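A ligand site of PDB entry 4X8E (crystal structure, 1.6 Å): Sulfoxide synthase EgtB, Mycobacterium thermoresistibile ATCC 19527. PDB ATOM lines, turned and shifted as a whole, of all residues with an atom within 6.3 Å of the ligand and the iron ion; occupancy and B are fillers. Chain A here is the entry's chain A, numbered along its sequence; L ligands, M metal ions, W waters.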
ATOM      1  N   TRP A  48      -7.888  -6.459  12.671  1.00  0.00           N
ATOM      2  CA  TRP A  48      -7.910  -6.347  11.225  1.00  0.00           C
ATOM      3  C   TRP A  48      -8.522  -7.636  10.635  1.00  0.00           C
ATOM      4  O   TRP A  48      -9.428  -7.575   9.772  1.00  0.00           O
ATOM      5  CB  TRP A  48      -6.504  -6.094  10.660  1.00  0.00           C
ATOM      6  CG  TRP A  48      -6.530  -5.848   9.158  1.00  0.00           C
ATOM      7  CD1 TRP A  48      -6.608  -4.641   8.526  1.00  0.00           C
ATOM      8  CD2 TRP A  48      -6.505  -6.844   8.109  1.00  0.00           C
ATOM      9  NE1 TRP A  48      -6.621  -4.817   7.168  1.00  0.00           N
ATOM     10  CE2 TRP A  48      -6.606  -6.154   6.888  1.00  0.00           C
ATOM     11  CE3 TRP A  48      -6.454  -8.241   8.097  1.00  0.00           C
ATOM     12  CZ2 TRP A  48      -6.591  -6.813   5.670  1.00  0.00           C
ATOM     13  CZ3 TRP A  48      -6.462  -8.888   6.894  1.00  0.00           C
ATOM     14  CH2 TRP A  48      -6.546  -8.180   5.701  1.00  0.00           C
ATOM     15  N   HIS A  52     -11.933  -7.978   8.422  1.00  0.00           N
ATOM     16  CA  HIS A  52     -11.691  -8.495   7.087  1.00  0.00           C
ATOM     17  C   HIS A  52     -12.522  -9.745   6.823  1.00  0.00           C
ATOM     18  O   HIS A  52     -13.083  -9.911   5.733  1.00  0.00           O
ATOM     19  CB  HIS A  52     -10.204  -8.835   6.919  1.00  0.00           C
ATOM     20  CG  HIS A  52      -9.889  -9.627   5.677  1.00  0.00           C
ATOM     21  ND1 HIS A  52      -9.649  -9.040   4.447  1.00  0.00           N
ATOM     22  CD2 HIS A  52      -9.734 -10.943   5.501  1.00  0.00           C
ATOM     23  CE1 HIS A  52      -9.363  -9.983   3.568  1.00  0.00           C
ATOM     24  NE2 HIS A  52      -9.408 -11.154   4.172  1.00  0.00           N
ATOM     25  N   GLN A  56     -15.269  -9.850   3.817  1.00  0.00           N
ATOM     26  CA  GLN A  56     -15.187 -10.836   2.763  1.00  0.00           C
ATOM     27  C   GLN A  56     -16.456 -11.675   2.734  1.00  0.00           C
ATOM     28  O   GLN A  56     -16.978 -11.991   1.666  1.00  0.00           O
ATOM     29  CB  GLN A  56     -13.949 -11.714   2.958  1.00  0.00           C
ATOM     30  CG  GLN A  56     -12.661 -10.941   2.650  1.00  0.00           C
ATOM     31  CD  GLN A  56     -12.387 -10.855   1.183  1.00  0.00           C
ATOM     32  OE1 GLN A  56     -12.076 -11.862   0.562  1.00  0.00           O
ATOM     33  NE2 GLN A  56     -12.570  -9.675   0.613  1.00  0.00           N
ATOM     34  N   ALA A  83      -6.213  -6.672   1.423  1.00  0.00           N
ATOM     35  CA  ALA A  83      -4.858  -7.118   1.684  1.00  0.00           C
ATOM     36  C   ALA A  83      -3.865  -6.744   0.597  1.00  0.00           C
ATOM     37  O   ALA A  83      -2.666  -6.699   0.858  1.00  0.00           O
ATOM     38  CB  ALA A  83      -4.846  -8.623   1.893  1.00  0.00           C
ATOM     39  N   ARG A  88       1.127  -5.967   5.304  1.00  0.00           N
ATOM     40  CA  ARG A  88       0.878  -6.393   6.678  1.00  0.00           C
ATOM     41  C   ARG A  88       1.360  -5.428   7.743  1.00  0.00           C
ATOM     42  O   ARG A  88       0.604  -5.102   8.661  1.00  0.00           O
ATOM     43  CB  ARG A  88       1.547  -7.749   6.910  1.00  0.00           C
ATOM     44  CG  ARG A  88       0.834  -8.942   6.293  1.00  0.00           C
ATOM     45  CD  ARG A  88      -0.168  -9.559   7.257  1.00  0.00           C
ATOM     46  NE  ARG A  88      -0.828 -10.746   6.708  1.00  0.00           N
ATOM     47  CZ  ARG A  88      -0.468 -12.003   6.922  1.00  0.00           C
ATOM     48  NH1 ARG A  88       0.575 -12.326   7.655  1.00  0.00           N
ATOM     49  NH2 ARG A  88      -1.184 -12.966   6.364  1.00  0.00           N
ATOM     50  N   HIS A 135     -12.293 -19.481   3.778  1.00  0.00           N
ATOM     51  CA  HIS A 135     -11.645 -18.183   3.995  1.00  0.00           C
ATOM     52  C   HIS A 135     -11.538 -17.835   5.499  1.00  0.00           C
ATOM     53  O   HIS A 135     -10.467 -17.455   5.976  1.00  0.00           O
ATOM     54  CB  HIS A 135     -12.423 -17.058   3.261  1.00  0.00           C
ATOM     55  CG  HIS A 135     -11.774 -15.720   3.428  1.00  0.00           C
ATOM     56  ND1 HIS A 135     -12.238 -14.772   4.318  1.00  0.00           N
ATOM     57  CD2 HIS A 135     -10.621 -15.229   2.927  1.00  0.00           C
ATOM     58  CE1 HIS A 135     -11.434 -13.723   4.307  1.00  0.00           C
ATOM     59  NE2 HIS A 135     -10.425 -13.969   3.469  1.00  0.00           N
ATOM     60  N   GLN A 138      -9.033 -20.100   7.301  1.00  0.00           N
ATOM     61  CA  GLN A 138      -7.662 -19.767   6.966  1.00  0.00           C
ATOM     62  C   GLN A 138      -7.190 -18.515   7.712  1.00  0.00           C
ATOM     63  O   GLN A 138      -6.041 -18.479   8.193  1.00  0.00           O
ATOM     64  CB  GLN A 138      -7.489 -19.604   5.448  1.00  0.00           C
ATOM     65  CG  GLN A 138      -7.680 -20.950   4.734  1.00  0.00           C
ATOM     66  CD  GLN A 138      -7.298 -20.887   3.285  1.00  0.00           C
ATOM     67  OE1 GLN A 138      -6.127 -20.700   2.957  1.00  0.00           O
ATOM     68  NE2 GLN A 138      -8.262 -21.030   2.390  1.00  0.00           N
ATOM     69  N   HIS A 139      -8.047 -17.518   7.860  1.00  0.00           N
ATOM     70  CA  HIS A 139      -7.669 -16.372   8.691  1.00  0.00           C
ATOM     71  C   HIS A 139      -7.557 -16.776  10.155  1.00  0.00           C
ATOM     72  O   HIS A 139      -6.769 -16.191  10.908  1.00  0.00           O
ATOM     73  CB  HIS A 139      -8.626 -15.209   8.512  1.00  0.00           C
ATOM     74  CG  HIS A 139      -8.308 -14.402   7.291  1.00  0.00           C
ATOM     75  ND1 HIS A 139      -7.423 -13.346   7.313  1.00  0.00           N
ATOM     76  CD2 HIS A 139      -8.698 -14.541   6.003  1.00  0.00           C
ATOM     77  CE1 HIS A 139      -7.283 -12.872   6.070  1.00  0.00           C
ATOM     78  NE2 HIS A 139      -8.062 -13.566   5.264  1.00  0.00           N
ATOM     79  N   THR A 142      -4.131 -17.856  10.449  1.00  0.00           N
ATOM     80  CA  THR A 142      -3.283 -16.672  10.486  1.00  0.00           C
ATOM     81  C   THR A 142      -3.278 -16.023  11.873  1.00  0.00           C
ATOM     82  O   THR A 142      -2.220 -15.644  12.390  1.00  0.00           O
ATOM     83  CB  THR A 142      -3.750 -15.657   9.423  1.00  0.00           C
ATOM     84  OG1 THR A 142      -3.598 -16.299   8.136  1.00  0.00           O
ATOM     85  CG2 THR A 142      -2.915 -14.397   9.496  1.00  0.00           C
ATOM     86  N   TYR A 378     -14.053 -15.402  -6.312  1.00  0.00           N
ATOM     87  CA  TYR A 378     -12.922 -14.660  -5.774  1.00  0.00           C
ATOM     88  C   TYR A 378     -11.734 -14.884  -6.719  1.00  0.00           C
ATOM     89  O   TYR A 378     -10.844 -15.726  -6.489  1.00  0.00           O
ATOM     90  CB  TYR A 378     -12.667 -15.114  -4.334  1.00  0.00           C
ATOM     91  CG  TYR A 378     -11.567 -14.445  -3.534  1.00  0.00           C
ATOM     92  CD1 TYR A 378     -10.771 -13.451  -4.082  1.00  0.00           C
ATOM     93  CD2 TYR A 378     -11.358 -14.818  -2.224  1.00  0.00           C
ATOM     94  CE1 TYR A 378      -9.763 -12.876  -3.337  1.00  0.00           C
ATOM     95  CE2 TYR A 378     -10.371 -14.243  -1.470  1.00  0.00           C
ATOM     96  CZ  TYR A 378      -9.566 -13.264  -2.031  1.00  0.00           C
ATOM     97  OH  TYR A 378      -8.579 -12.689  -1.276  1.00  0.00           O
ATOM     98  N   TYR A 381      -7.967 -14.833  -5.673  1.00  0.00           N
ATOM     99  CA  TYR A 381      -7.532 -15.724  -4.600  1.00  0.00           C
ATOM    100  C   TYR A 381      -6.222 -16.460  -4.948  1.00  0.00           C
ATOM    101  O   TYR A 381      -5.318 -16.528  -4.101  1.00  0.00           O
ATOM    102  CB  TYR A 381      -8.622 -16.753  -4.285  1.00  0.00           C
ATOM    103  CG  TYR A 381      -8.205 -17.746  -3.214  1.00  0.00           C
ATOM    104  CD1 TYR A 381      -8.315 -17.466  -1.846  1.00  0.00           C
ATOM    105  CD2 TYR A 381      -7.695 -18.965  -3.559  1.00  0.00           C
ATOM    106  CE1 TYR A 381      -7.925 -18.370  -0.884  1.00  0.00           C
ATOM    107  CE2 TYR A 381      -7.322 -19.868  -2.602  1.00  0.00           C
ATOM    108  CZ  TYR A 381      -7.417 -19.575  -1.281  1.00  0.00           C
ATOM    109  OH  TYR A 381      -6.986 -20.499  -0.359  1.00  0.00           O
ATOM    110  N   PHE A 385      -0.719 -15.088  -7.585  1.00  0.00           N
ATOM    111  CA  PHE A 385       0.400 -15.742  -6.937  1.00  0.00           C
ATOM    112  C   PHE A 385       0.982 -16.858  -7.774  1.00  0.00           C
ATOM    113  O   PHE A 385       1.936 -17.517  -7.355  1.00  0.00           O
ATOM    114  CB  PHE A 385      -0.046 -16.229  -5.544  1.00  0.00           C
ATOM    115  CG  PHE A 385      -0.780 -15.154  -4.792  1.00  0.00           C
ATOM    116  CD1 PHE A 385      -0.097 -14.027  -4.371  1.00  0.00           C
ATOM    117  CD2 PHE A 385      -2.161 -15.203  -4.620  1.00  0.00           C
ATOM    118  CE1 PHE A 385      -0.774 -12.973  -3.750  1.00  0.00           C
ATOM    119  CE2 PHE A 385      -2.835 -14.154  -3.991  1.00  0.00           C
ATOM    120  CZ  PHE A 385      -2.127 -13.049  -3.556  1.00  0.00           C
ATOM    121  N   PHE A 413      -5.816 -29.740  -1.608  1.00  0.00           N
ATOM    122  CA  PHE A 413      -5.702 -28.352  -1.168  1.00  0.00           C
ATOM    123  C   PHE A 413      -4.272 -27.836  -1.301  1.00  0.00           C
ATOM    124  O   PHE A 413      -3.326 -28.544  -0.967  1.00  0.00           O
ATOM    125  CB  PHE A 413      -6.184 -28.190   0.303  1.00  0.00           C
ATOM    126  CG  PHE A 413      -6.254 -26.764   0.740  1.00  0.00           C
ATOM    127  CD1 PHE A 413      -5.102 -26.112   1.170  1.00  0.00           C
ATOM    128  CD2 PHE A 413      -7.452 -26.073   0.654  1.00  0.00           C
ATOM    129  CE1 PHE A 413      -5.137 -24.770   1.533  1.00  0.00           C
ATOM    130  CE2 PHE A 413      -7.519 -24.727   1.044  1.00  0.00           C
ATOM    131  CZ  PHE A 413      -6.347 -24.075   1.466  1.00  0.00           C
ATOM    132  N   ARG A 414      -4.136 -26.598  -1.792  1.00  0.00           N
ATOM    133  CA  ARG A 414      -2.832 -26.002  -2.013  1.00  0.00           C
ATOM    134  C   ARG A 414      -2.661 -24.735  -1.190  1.00  0.00           C
ATOM    135  O   ARG A 414      -3.362 -23.755  -1.415  1.00  0.00           O
ATOM    136  CB  ARG A 414      -2.637 -25.687  -3.489  1.00  0.00           C
ATOM    137  CG  ARG A 414      -2.894 -26.910  -4.375  1.00  0.00           C
ATOM    138  CD  ARG A 414      -2.958 -26.589  -5.856  1.00  0.00           C
ATOM    139  NE  ARG A 414      -1.650 -26.323  -6.435  1.00  0.00           N
ATOM    140  CZ  ARG A 414      -1.479 -25.783  -7.629  1.00  0.00           C
ATOM    141  NH1 ARG A 414      -2.506 -25.407  -8.362  1.00  0.00           N
ATOM    142  NH2 ARG A 414      -0.246 -25.616  -8.102  1.00  0.00           N
ATOM    143  N   ASN A 415      -1.745 -24.752  -0.234  1.00  0.00           N
ATOM    144  CA  ASN A 415      -1.286 -23.537   0.447  1.00  0.00           C
ATOM    145  C   ASN A 415      -0.030 -23.064  -0.274  1.00  0.00           C
ATOM    146  O   ASN A 415       0.549 -23.818  -1.062  1.00  0.00           O
ATOM    147  CB  ASN A 415      -1.036 -23.883   1.926  1.00  0.00           C
ATOM    148  CG  ASN A 415      -0.660 -22.711   2.809  1.00  0.00           C
ATOM    149  OD1 ASN A 415      -0.822 -21.519   2.469  1.00  0.00           O
ATOM    150  ND2 ASN A 415      -0.207 -23.074   4.017  1.00  0.00           N
ATOM    151  N   TRP A 416       0.395 -21.833  -0.032  1.00  0.00           N
ATOM    152  CA  TRP A 416       1.633 -21.334  -0.610  1.00  0.00           C
ATOM    153  C   TRP A 416       2.116 -20.165   0.218  1.00  0.00           C
ATOM    154  O   TRP A 416       1.341 -19.465   0.906  1.00  0.00           O
ATOM    155  CB  TRP A 416       1.441 -20.893  -2.082  1.00  0.00           C
ATOM    156  CG  TRP A 416       0.485 -19.748  -2.248  1.00  0.00           C
ATOM    157  CD1 TRP A 416       0.797 -18.429  -2.253  1.00  0.00           C
ATOM    158  CD2 TRP A 416      -0.946 -19.817  -2.433  1.00  0.00           C
ATOM    159  NE1 TRP A 416      -0.336 -17.668  -2.398  1.00  0.00           N
ATOM    160  CE2 TRP A 416      -1.423 -18.491  -2.525  1.00  0.00           C
ATOM    161  CE3 TRP A 416      -1.863 -20.879  -2.531  1.00  0.00           C
ATOM    162  CZ2 TRP A 416      -2.781 -18.180  -2.704  1.00  0.00           C
ATOM    163  CZ3 TRP A 416      -3.227 -20.576  -2.712  1.00  0.00           C
ATOM    164  CH2 TRP A 416      -3.666 -19.227  -2.807  1.00  0.00           C
ATOM    165  N   ASP A 417       3.421 -19.938   0.176  1.00  0.00           N
ATOM    166  CA  ASP A 417       3.962 -18.761   0.815  1.00  0.00           C
ATOM    167  C   ASP A 417       5.331 -18.429   0.249  1.00  0.00           C
ATOM    168  O   ASP A 417       5.954 -19.232  -0.438  1.00  0.00           O
ATOM    169  CB  ASP A 417       4.030 -18.970   2.346  1.00  0.00           C
ATOM    170  CG  ASP A 417       3.667 -17.713   3.093  1.00  0.00           C
ATOM    171  OD1 ASP A 417       4.013 -16.582   2.641  1.00  0.00           O
ATOM    172  OD2 ASP A 417       2.945 -17.839   4.118  1.00  0.00           O
HETATM  173  C1  LIG L   1      -3.692 -19.550   0.883  1.00  0.00           C
HETATM  174  C2  LIG L   1      -3.200 -19.161   3.196  1.00  0.00           C
HETATM  175  C3  LIG L   1      -1.874 -18.234   1.454  1.00  0.00           C
HETATM  176  O1  LIG L   1      -3.151 -15.186   2.094  1.00  0.00           O
HETATM  177  O2  LIG L   1      -3.574 -16.322   3.922  1.00  0.00           O
HETATM  178  C4  LIG L   1      -7.063 -15.651   3.033  1.00  0.00           C
HETATM  179  C5  LIG L   1      -5.573 -17.635   2.185  1.00  0.00           C
HETATM  180  N1  LIG L   1      -6.493 -15.650   0.854  1.00  0.00           N
HETATM  181  N2  LIG L   1      -7.609 -14.539   2.408  1.00  0.00           N
HETATM  182  C6  LIG L   1      -3.575 -16.237   2.659  1.00  0.00           C
HETATM  183  C7  LIG L   1      -6.381 -16.326   2.042  1.00  0.00           C
HETATM  184  C8  LIG L   1      -7.279 -14.526   1.096  1.00  0.00           C
HETATM  185  C9  LIG L   1      -4.112 -17.345   1.802  1.00  0.00           C
HETATM  186  N3  LIG L   1      -3.230 -18.542   1.847  1.00  0.00           N
HETATM  187 FE    FE M   1      -8.642 -12.951   3.338  1.00  0.00          FE
HETATM  188  O   HOH W   1      -2.958 -14.604  -0.506  1.00  0.00           O
HETATM  189  O   HOH W   2      -9.368 -12.205   1.385  1.00  0.00           O
HETATM  190  O   HOH W   3      -6.900 -11.847   3.004  1.00  0.00           O
HETATM  191  O   HOH W   4      -3.842 -18.978   6.418  1.00  0.00           O
HETATM  192  O   HOH W   5      -0.420 -14.683   2.866  1.00  0.00           O
HETATM  193  O   HOH W   6      -4.250 -12.750   2.693  1.00  0.00           O
HETATM  194  O   HOH W   7       0.956 -16.588   0.905  1.00  0.00           O
HETATM  195  O   HOH W   8      -5.242 -15.662  -1.574  1.00  0.00           O
HETATM  196  O   HOH W   9      -4.329 -14.829   6.038  1.00  0.00           O
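O of Gln 138 sits at hydrogen-bond distance from OG1 of Thr 142, 3.3 Å away.
The side-chain amide nitrogen of Gln 138 lies within hydrogen-bond range of the side-chain hydroxyl of Tyr 381.
Merely in contact with the ligand: Gln 138 (3.2 Å), Tyr 378 (3.3 Å), Tyr 381 (3.5 Å), Asn 415 (3.4 Å) and Trp 416 (3.5 Å).
Hydrophobic or aromatic side chains within 4 Å of the ligand: His 135, His 139, Tyr 381 and Trp 416.
Seven residues have an atom within 4 Å of the ligand: His 135, Gln 138, His 139, Tyr 378, Tyr 381, Asn 415 and Trp 416.
Three residues have an atom within 4 Å of the iron ion: His 52, His 135 and His 139.
The iron ion is bound by NE2 of His 135, water W3, NE2 of His 139, N2 of the ligand, NE2 of His 52 and water W2.
Water W2 bridges OH of Tyr 378 (2.8 Å) and OE1 of Gln 56 (2.9 Å).
Water W9 bridges the side-chain hydroxyl (OG1) of Thr 142 (2.7 Å) and an oxygen (O2) of the ligand (2.7 Å).
Water W8 bridges the backbone carbonyl oxygen of Tyr 381 (2.7 Å) and a nitrogen (N1) of the ligand (2.7 Å).
Water W4 lies within hydrogen-bond range of O of Gln 138 and OG1 of Thr 142.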
